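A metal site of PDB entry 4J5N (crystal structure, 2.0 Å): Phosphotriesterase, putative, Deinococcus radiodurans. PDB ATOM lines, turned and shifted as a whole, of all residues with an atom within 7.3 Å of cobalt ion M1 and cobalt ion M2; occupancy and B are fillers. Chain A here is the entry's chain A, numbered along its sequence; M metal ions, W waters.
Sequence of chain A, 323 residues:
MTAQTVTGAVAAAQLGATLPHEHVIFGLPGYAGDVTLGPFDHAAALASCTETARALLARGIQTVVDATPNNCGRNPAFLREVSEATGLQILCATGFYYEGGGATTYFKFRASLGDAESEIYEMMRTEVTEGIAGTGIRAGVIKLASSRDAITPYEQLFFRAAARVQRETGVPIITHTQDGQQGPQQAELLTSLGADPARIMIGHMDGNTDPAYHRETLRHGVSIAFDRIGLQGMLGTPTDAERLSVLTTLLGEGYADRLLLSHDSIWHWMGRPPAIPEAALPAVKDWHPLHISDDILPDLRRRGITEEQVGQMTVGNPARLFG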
ATOM      1  N   HIS A  21      17.722 -10.067 -13.235  1.00  0.00           N
ATOM      2  CA  HIS A  21      16.258 -10.013 -13.241  1.00  0.00           C
ATOM      3  C   HIS A  21      15.745  -8.573 -13.480  1.00  0.00           C
ATOM      4  O   HIS A  21      15.685  -7.783 -12.541  1.00  0.00           O
ATOM      5  CB  HIS A  21      15.713 -10.536 -11.901  1.00  0.00           C
ATOM      6  CG  HIS A  21      14.254 -10.854 -11.892  1.00  0.00           C
ATOM      7  ND1 HIS A  21      13.766 -12.097 -11.549  1.00  0.00           N
ATOM      8  CD2 HIS A  21      13.159 -10.098 -12.162  1.00  0.00           C
ATOM      9  CE1 HIS A  21      12.457 -12.098 -11.603  1.00  0.00           C
ATOM     10  NE2 HIS A  21      12.060 -10.885 -11.976  1.00  0.00           N
ATOM     11  N   GLU A  22      15.372  -8.271 -14.721  1.00  0.00           N
ATOM     12  CA  GLU A  22      14.819  -6.961 -15.091  1.00  0.00           C
ATOM     13  C   GLU A  22      13.743  -7.180 -16.151  1.00  0.00           C
ATOM     14  O   GLU A  22      13.590  -8.301 -16.653  1.00  0.00           O
ATOM     15  CB  GLU A  22      15.885  -6.021 -15.692  1.00  0.00           C
ATOM     16  CG  GLU A  22      17.150  -5.746 -14.866  1.00  0.00           C
ATOM     17  CD  GLU A  22      16.905  -5.109 -13.502  1.00  0.00           C
ATOM     18  OE1 GLU A  22      15.916  -4.366 -13.326  1.00  0.00           O
ATOM     19  OE2 GLU A  22      17.721  -5.351 -12.580  1.00  0.00           O
ATOM     20  N   HIS A  23      12.965  -6.143 -16.451  1.00  0.00           N
ATOM     21  CA  HIS A  23      11.923  -6.234 -17.486  1.00  0.00           C
ATOM     22  C   HIS A  23      12.002  -5.021 -18.401  1.00  0.00           C
ATOM     23  O   HIS A  23      11.728  -3.907 -17.961  1.00  0.00           O
ATOM     24  CB  HIS A  23      10.519  -6.291 -16.864  1.00  0.00           C
ATOM     25  CG  HIS A  23      10.325  -7.407 -15.879  1.00  0.00           C
ATOM     26  ND1 HIS A  23      10.067  -8.708 -16.268  1.00  0.00           N
ATOM     27  CD2 HIS A  23      10.387  -7.422 -14.529  1.00  0.00           C
ATOM     28  CE1 HIS A  23       9.985  -9.467 -15.193  1.00  0.00           C
ATOM     29  NE2 HIS A  23      10.178  -8.712 -14.132  1.00  0.00           N
ATOM     30  N   PHE A  26       6.893  -4.849 -19.632  1.00  0.00           N
ATOM     31  CA  PHE A  26       6.086  -5.708 -18.768  1.00  0.00           C
ATOM     32  C   PHE A  26       4.664  -5.202 -18.711  1.00  0.00           C
ATOM     33  O   PHE A  26       4.398  -3.990 -18.562  1.00  0.00           O
ATOM     34  CB  PHE A  26       6.674  -5.759 -17.340  1.00  0.00           C
ATOM     35  CG  PHE A  26       6.047  -6.795 -16.415  1.00  0.00           C
ATOM     36  CD1 PHE A  26       4.923  -6.475 -15.608  1.00  0.00           C
ATOM     37  CD2 PHE A  26       6.617  -8.076 -16.292  1.00  0.00           C
ATOM     38  CE1 PHE A  26       4.389  -7.417 -14.685  1.00  0.00           C
ATOM     39  CE2 PHE A  26       6.088  -9.040 -15.376  1.00  0.00           C
ATOM     40  CZ  PHE A  26       4.975  -8.710 -14.573  1.00  0.00           C
ATOM     41  N   ALA A  67      13.400 -11.221 -17.349  1.00  0.00           N
ATOM     42  CA  ALA A  67      12.634 -12.270 -16.696  1.00  0.00           C
ATOM     43  C   ALA A  67      11.151 -12.323 -16.997  1.00  0.00           C
ATOM     44  O   ALA A  67      10.427 -13.078 -16.332  1.00  0.00           O
ATOM     45  CB  ALA A  67      12.848 -12.166 -15.223  1.00  0.00           C
ATOM     46  N   THR A  68      10.716 -11.569 -18.000  1.00  0.00           N
ATOM     47  CA  THR A  68       9.300 -11.483 -18.377  1.00  0.00           C
ATOM     48  C   THR A  68       8.637 -12.794 -18.828  1.00  0.00           C
ATOM     49  O   THR A  68       9.051 -13.384 -19.834  1.00  0.00           O
ATOM     50  CB  THR A  68       9.072 -10.373 -19.468  1.00  0.00           C
ATOM     51  OG1 THR A  68       9.789  -9.197 -19.079  1.00  0.00           O
ATOM     52  CG2 THR A  68       7.600 -10.028 -19.591  1.00  0.00           C
ATOM     53  N   PRO A  69       7.612 -13.260 -18.081  1.00  0.00           N
ATOM     54  CA  PRO A  69       6.881 -14.495 -18.402  1.00  0.00           C
ATOM     55  C   PRO A  69       6.077 -14.335 -19.690  1.00  0.00           C
ATOM     56  O   PRO A  69       5.702 -13.211 -20.053  1.00  0.00           O
ATOM     57  CB  PRO A  69       5.949 -14.661 -17.200  1.00  0.00           C
ATOM     58  CG  PRO A  69       6.717 -14.019 -16.077  1.00  0.00           C
ATOM     59  CD  PRO A  69       7.220 -12.777 -16.744  1.00  0.00           C
ATOM     60  N   TYR A  97       3.651 -16.904 -15.218  1.00  0.00           N
ATOM     61  CA  TYR A  97       3.648 -16.250 -13.914  1.00  0.00           C
ATOM     62  C   TYR A  97       2.901 -17.118 -12.873  1.00  0.00           C
ATOM     63  O   TYR A  97       2.341 -18.160 -13.226  1.00  0.00           O
ATOM     64  CB  TYR A  97       2.992 -14.861 -14.054  1.00  0.00           C
ATOM     65  CG  TYR A  97       3.504 -13.748 -13.162  1.00  0.00           C
ATOM     66  CD1 TYR A  97       4.856 -13.672 -12.770  1.00  0.00           C
ATOM     67  CD2 TYR A  97       2.634 -12.703 -12.761  1.00  0.00           C
ATOM     68  CE1 TYR A  97       5.347 -12.572 -11.997  1.00  0.00           C
ATOM     69  CE2 TYR A  97       3.112 -11.598 -11.985  1.00  0.00           C
ATOM     70  CZ  TYR A  97       4.474 -11.542 -11.613  1.00  0.00           C
ATOM     71  OH  TYR A  97       4.953 -10.487 -10.876  1.00  0.00           O
ATOM     72  N   TYR A  98       2.882 -16.675 -11.606  1.00  0.00           N
ATOM     73  CA  TYR A  98       2.208 -17.424 -10.528  1.00  0.00           C
ATOM     74  C   TYR A  98       0.667 -17.456 -10.669  1.00  0.00           C
ATOM     75  O   TYR A  98       0.090 -16.642 -11.382  1.00  0.00           O
ATOM     76  CB  TYR A  98       2.674 -16.936  -9.133  1.00  0.00           C
ATOM     77  CG  TYR A  98       2.185 -15.576  -8.658  1.00  0.00           C
ATOM     78  CD1 TYR A  98       2.531 -14.382  -9.342  1.00  0.00           C
ATOM     79  CD2 TYR A  98       1.340 -15.478  -7.527  1.00  0.00           C
ATOM     80  CE1 TYR A  98       2.031 -13.118  -8.912  1.00  0.00           C
ATOM     81  CE2 TYR A  98       0.839 -14.222  -7.090  1.00  0.00           C
ATOM     82  CZ  TYR A  98       1.181 -13.050  -7.784  1.00  0.00           C
ATOM     83  OH  TYR A  98       0.658 -11.840  -7.386  1.00  0.00           O
ATOM     84  N   KCX A 143      11.710 -19.170 -16.614  1.00  0.00           N
ATOM     85  CA  KCX A 143      11.171 -18.406 -15.486  1.00  0.00           C
ATOM     86  CB  KCX A 143      10.592 -17.081 -16.006  1.00  0.00           C
ATOM     87  CG  KCX A 143       9.874 -16.275 -14.937  1.00  0.00           C
ATOM     88  CD  KCX A 143      10.801 -15.893 -13.771  1.00  0.00           C
ATOM     89  CE  KCX A 143      10.081 -14.981 -12.780  1.00  0.00           C
ATOM     90  NZ  KCX A 143       9.734 -13.699 -13.425  1.00  0.00           N
ATOM     91  C   KCX A 143      10.070 -19.229 -14.809  1.00  0.00           C
ATOM     92  O   KCX A 143       9.135 -19.684 -15.450  1.00  0.00           O
ATOM     93  CX  KCX A 143       9.349 -12.635 -12.733  1.00  0.00           C
ATOM     94  OQ1 KCX A 143       9.276 -12.724 -11.485  1.00  0.00           O
ATOM     95  OQ2 KCX A 143       9.091 -11.589 -13.366  1.00  0.00           O
ATOM     96  N   LEU A 144      10.202 -19.399 -13.495  1.00  0.00           N
ATOM     97  CA  LEU A 144       9.232 -20.121 -12.688  1.00  0.00           C
ATOM     98  C   LEU A 144       8.727 -19.201 -11.609  1.00  0.00           C
ATOM     99  O   LEU A 144       9.440 -18.311 -11.159  1.00  0.00           O
ATOM    100  CB  LEU A 144       9.881 -21.353 -12.043  1.00  0.00           C
ATOM    101  CG  LEU A 144      10.330 -22.488 -12.948  1.00  0.00           C
ATOM    102  CD1 LEU A 144      11.008 -23.549 -12.129  1.00  0.00           C
ATOM    103  CD2 LEU A 144       9.131 -23.059 -13.698  1.00  0.00           C
ATOM    104  N   ALA A 145       7.490 -19.419 -11.176  1.00  0.00           N
ATOM    105  CA  ALA A 145       6.887 -18.602 -10.135  1.00  0.00           C
ATOM    106  C   ALA A 145       5.987 -19.426  -9.234  1.00  0.00           C
ATOM    107  O   ALA A 145       5.362 -20.386  -9.687  1.00  0.00           O
ATOM    108  CB  ALA A 145       6.106 -17.484 -10.777  1.00  0.00           C
ATOM    109  N   THR A 175      13.684 -17.740 -10.763  1.00  0.00           N
ATOM    110  CA  THR A 175      12.343 -17.795 -10.202  1.00  0.00           C
ATOM    111  C   THR A 175      11.808 -16.506  -9.559  1.00  0.00           C
ATOM    112  O   THR A 175      12.547 -15.558  -9.336  1.00  0.00           O
ATOM    113  CB  THR A 175      12.193 -18.924  -9.121  1.00  0.00           C
ATOM    114  OG1 THR A 175      12.688 -18.440  -7.873  1.00  0.00           O
ATOM    115  CG2 THR A 175      12.919 -20.222  -9.506  1.00  0.00           C
ATOM    116  N   HIS A 176      10.528 -16.568  -9.201  1.00  0.00           N
ATOM    117  CA  HIS A 176       9.792 -15.518  -8.509  1.00  0.00           C
ATOM    118  C   HIS A 176       9.270 -16.182  -7.227  1.00  0.00           C
ATOM    119  O   HIS A 176       8.762 -17.305  -7.289  1.00  0.00           O
ATOM    120  CB  HIS A 176       8.615 -15.020  -9.408  1.00  0.00           C
ATOM    121  CG  HIS A 176       7.468 -14.360  -8.669  1.00  0.00           C
ATOM    122  ND1 HIS A 176       7.321 -12.993  -8.600  1.00  0.00           N
ATOM    123  CD2 HIS A 176       6.414 -14.890  -7.994  1.00  0.00           C
ATOM    124  CE1 HIS A 176       6.233 -12.697  -7.917  1.00  0.00           C
ATOM    125  NE2 HIS A 176       5.659 -13.832  -7.531  1.00  0.00           N
ATOM    126  N   THR A 177       9.404 -15.487  -6.092  1.00  0.00           N
ATOM    127  CA  THR A 177       8.842 -15.942  -4.829  1.00  0.00           C
ATOM    128  C   THR A 177       7.893 -14.824  -4.392  1.00  0.00           C
ATOM    129  O   THR A 177       8.210 -13.634  -4.526  1.00  0.00           O
ATOM    130  CB  THR A 177       9.888 -16.201  -3.696  1.00  0.00           C
ATOM    131  OG1 THR A 177      10.761 -15.088  -3.541  1.00  0.00           O
ATOM    132  CG2 THR A 177      10.692 -17.463  -3.986  1.00  0.00           C
ATOM    133  N   GLN A 178       6.706 -15.213  -3.928  1.00  0.00           N
ATOM    134  CA  GLN A 178       5.701 -14.247  -3.502  1.00  0.00           C
ATOM    135  C   GLN A 178       5.741 -13.985  -2.006  1.00  0.00           C
ATOM    136  O   GLN A 178       5.747 -14.919  -1.192  1.00  0.00           O
ATOM    137  CB  GLN A 178       4.309 -14.738  -3.947  1.00  0.00           C
ATOM    138  CG  GLN A 178       3.132 -13.789  -3.699  1.00  0.00           C
ATOM    139  CD  GLN A 178       3.166 -12.526  -4.568  1.00  0.00           C
ATOM    140  OE1 GLN A 178       3.762 -12.514  -5.651  1.00  0.00           O
ATOM    141  NE2 GLN A 178       2.505 -11.474  -4.096  1.00  0.00           N
ATOM    142  N   GLY A 203      14.592 -16.310  -6.946  1.00  0.00           N
ATOM    143  CA  GLY A 203      14.385 -14.868  -6.895  1.00  0.00           C
ATOM    144  C   GLY A 203      13.533 -14.333  -5.770  1.00  0.00           C
ATOM    145  O   GLY A 203      12.943 -15.108  -5.016  1.00  0.00           O
ATOM    146  N   HIS A 204      13.459 -12.998  -5.709  1.00  0.00           N
ATOM    147  CA  HIS A 204      12.714 -12.211  -4.709  1.00  0.00           C
ATOM    148  C   HIS A 204      13.018 -12.616  -3.279  1.00  0.00           C
ATOM    149  O   HIS A 204      12.187 -12.475  -2.366  1.00  0.00           O
ATOM    150  CB  HIS A 204      11.202 -12.190  -4.994  1.00  0.00           C
ATOM    151  CG  HIS A 204      10.838 -11.795  -6.400  1.00  0.00           C
ATOM    152  ND1 HIS A 204      11.730 -11.223  -7.277  1.00  0.00           N
ATOM    153  CD2 HIS A 204       9.689 -11.949  -7.093  1.00  0.00           C
ATOM    154  CE1 HIS A 204      11.154 -11.060  -8.450  1.00  0.00           C
ATOM    155  NE2 HIS A 204       9.912 -11.491  -8.365  1.00  0.00           N
ATOM    156  N   ASP A 227      16.755  -9.427  -5.767  1.00  0.00           N
ATOM    157  CA  ASP A 227      16.375  -8.832  -7.035  1.00  0.00           C
ATOM    158  C   ASP A 227      15.306  -7.755  -7.163  1.00  0.00           C
ATOM    159  O   ASP A 227      14.892  -7.457  -8.284  1.00  0.00           O
ATOM    160  CB  ASP A 227      16.170  -9.940  -8.077  1.00  0.00           C
ATOM    161  CG  ASP A 227      15.048 -10.907  -7.735  1.00  0.00           C
ATOM    162  OD1 ASP A 227      14.197 -10.549  -6.902  1.00  0.00           O
ATOM    163  OD2 ASP A 227      15.027 -12.021  -8.282  1.00  0.00           O
ATOM    164  N   ARG A 228      14.813  -7.213  -6.059  1.00  0.00           N
ATOM    165  CA  ARG A 228      13.816  -6.144  -6.111  1.00  0.00           C
ATOM    166  C   ARG A 228      14.403  -4.921  -5.398  1.00  0.00           C
ATOM    167  O   ARG A 228      13.689  -4.155  -4.755  1.00  0.00           O
ATOM    168  CB  ARG A 228      12.465  -6.572  -5.495  1.00  0.00           C
ATOM    169  CG  ARG A 228      11.937  -7.919  -5.977  1.00  0.00           C
ATOM    170  CD  ARG A 228      10.488  -8.130  -5.616  1.00  0.00           C
ATOM    171  NE  ARG A 228       9.602  -7.506  -6.582  1.00  0.00           N
ATOM    172  CZ  ARG A 228       8.267  -7.560  -6.535  1.00  0.00           C
ATOM    173  NH1 ARG A 228       7.656  -8.220  -5.559  1.00  0.00           N
ATOM    174  NH2 ARG A 228       7.542  -6.952  -7.463  1.00  0.00           N
ATOM    175  N   HIS A 263      17.137  -5.311  -9.848  1.00  0.00           N
ATOM    176  CA  HIS A 263      16.091  -4.373  -9.414  1.00  0.00           C
ATOM    177  C   HIS A 263      14.658  -4.790  -9.653  1.00  0.00           C
ATOM    178  O   HIS A 263      13.760  -4.298  -8.965  1.00  0.00           O
ATOM    179  CB  HIS A 263      16.247  -3.002 -10.102  1.00  0.00           C
ATOM    180  CG  HIS A 263      17.648  -2.486 -10.130  1.00  0.00           C
ATOM    181  ND1 HIS A 263      18.538  -2.819 -11.121  1.00  0.00           N
ATOM    182  CD2 HIS A 263      18.301  -1.652  -9.292  1.00  0.00           C
ATOM    183  CE1 HIS A 263      19.685  -2.206 -10.895  1.00  0.00           C
ATOM    184  NE2 HIS A 263      19.569  -1.487  -9.791  1.00  0.00           N
ATOM    185  N   ASP A 264      14.429  -5.686 -10.635  1.00  0.00           N
ATOM    186  CA  ASP A 264      13.085  -6.140 -11.048  1.00  0.00           C
ATOM    187  C   ASP A 264      12.313  -4.912 -11.585  1.00  0.00           C
ATOM    188  O   ASP A 264      11.083  -4.796 -11.427  1.00  0.00           O
ATOM    189  CB  ASP A 264      12.311  -6.840  -9.890  1.00  0.00           C
ATOM    190  CG  ASP A 264      11.072  -7.586 -10.377  1.00  0.00           C
ATOM    191  OD1 ASP A 264      10.968  -7.870 -11.582  1.00  0.00           O
ATOM    192  OD2 ASP A 264      10.178  -7.865  -9.540  1.00  0.00           O
ATOM    193  N   SER A 265      13.069  -4.016 -12.225  1.00  0.00           N
ATOM    194  CA  SER A 265      12.534  -2.778 -12.801  1.00  0.00           C
ATOM    195  C   SER A 265      11.777  -3.025 -14.090  1.00  0.00           C
ATOM    196  O   SER A 265      11.965  -4.049 -14.758  1.00  0.00           O
ATOM    197  CB  SER A 265      13.674  -1.792 -13.077  1.00  0.00           C
ATOM    198  OG  SER A 265      14.491  -2.231 -14.149  1.00  0.00           O
ATOM    199  N   ILE A 266      10.897  -2.092 -14.415  1.00  0.00           N
ATOM    200  CA  ILE A 266      10.097  -2.159 -15.636  1.00  0.00           C
ATOM    201  C   ILE A 266      10.432  -0.860 -16.372  1.00  0.00           C
ATOM    202  O   ILE A 266      10.141   0.231 -15.871  1.00  0.00           O
ATOM    203  CB  ILE A 266       8.591  -2.301 -15.299  1.00  0.00           C
ATOM    204  CG1 ILE A 266       8.354  -3.642 -14.577  1.00  0.00           C
ATOM    205  CG2 ILE A 266       7.755  -2.254 -16.594  1.00  0.00           C
ATOM    206  CD1 ILE A 266       7.072  -3.764 -13.812  1.00  0.00           C
HETATM  207 CO    CO M   1      10.126  -9.767 -12.409  1.00  0.00          CO
HETATM  208 CO    CO M   2       8.444 -11.643  -9.845  1.00  0.00          CO
HETATM  209  O   HOH W   1       7.291  -9.895  -8.531  1.00  0.00           O
HETATM  210  O   HOH W   2       7.259  -8.432 -12.013  1.00  0.00           O
HETATM  211  O   HOH W   3       9.156  -9.757 -10.966  1.00  0.00           O
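A ring nitrogen (ND1) of His 23 is in hydrogen-bond range of the side-chain hydroxyl (OG1) of Thr 68, at 2.9 Å. The backbone carbonyl oxygen of Ser 265 is in hydrogen-bond range of the backbone NH of His 23 (2.9 Å). O of His 204 sits at hydrogen-bond distance from OG1 of Thr 177. NZ of KCX 143 is in hydrogen-bond range of the backbone carbonyl oxygen (O) of Ala 67, at 3.1 Å. A ring nitrogen (NE2) of His 176 sits at hydrogen-bond distance from the side-chain amide oxygen (OE1) of Gln 178 (3.0 Å). O of Leu 144 sits at hydrogen-bond distance from N of His 176, at 2.8 Å. OD2 of Asp 264 lies within salt-bridge range of NE of Arg 228 (3.0 Å). The backbone NH (N) of Asp 264 lies within hydrogen-bond range of the backbone carbonyl oxygen (O) of Asp 227 (3.0 Å).
Tyr 97 touches cobalt ion M2.
Cobalt ion M1 is bound by water W3 (1.7 Å), a ring nitrogen (NE2) of His 23 (2.0 Å), the side-chain carboxylate (OD1) of Asp 264 (2.2 Å), a ring nitrogen (NE2) of His 21 (2.3 Å) and OQ2 of KCX 143 (2.3 Å).
NE2 of His 204 is bound to cobalt ion M2, 2.1 Å away. OQ1 of KCX 143 binds cobalt ion M2 (2.1 Å). Cobalt ion M2 is bound by ND1 of His 176 (2.2 Å). Cobalt ion M2 is bound by water W3 (2.3 Å). Water W1 binds cobalt ion M2, at 2.5 Å.
Water W1 lies within hydrogen-bond range of NH2 of Arg 228 (3.1 Å) and OH of Tyr 97 (3.4 Å).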
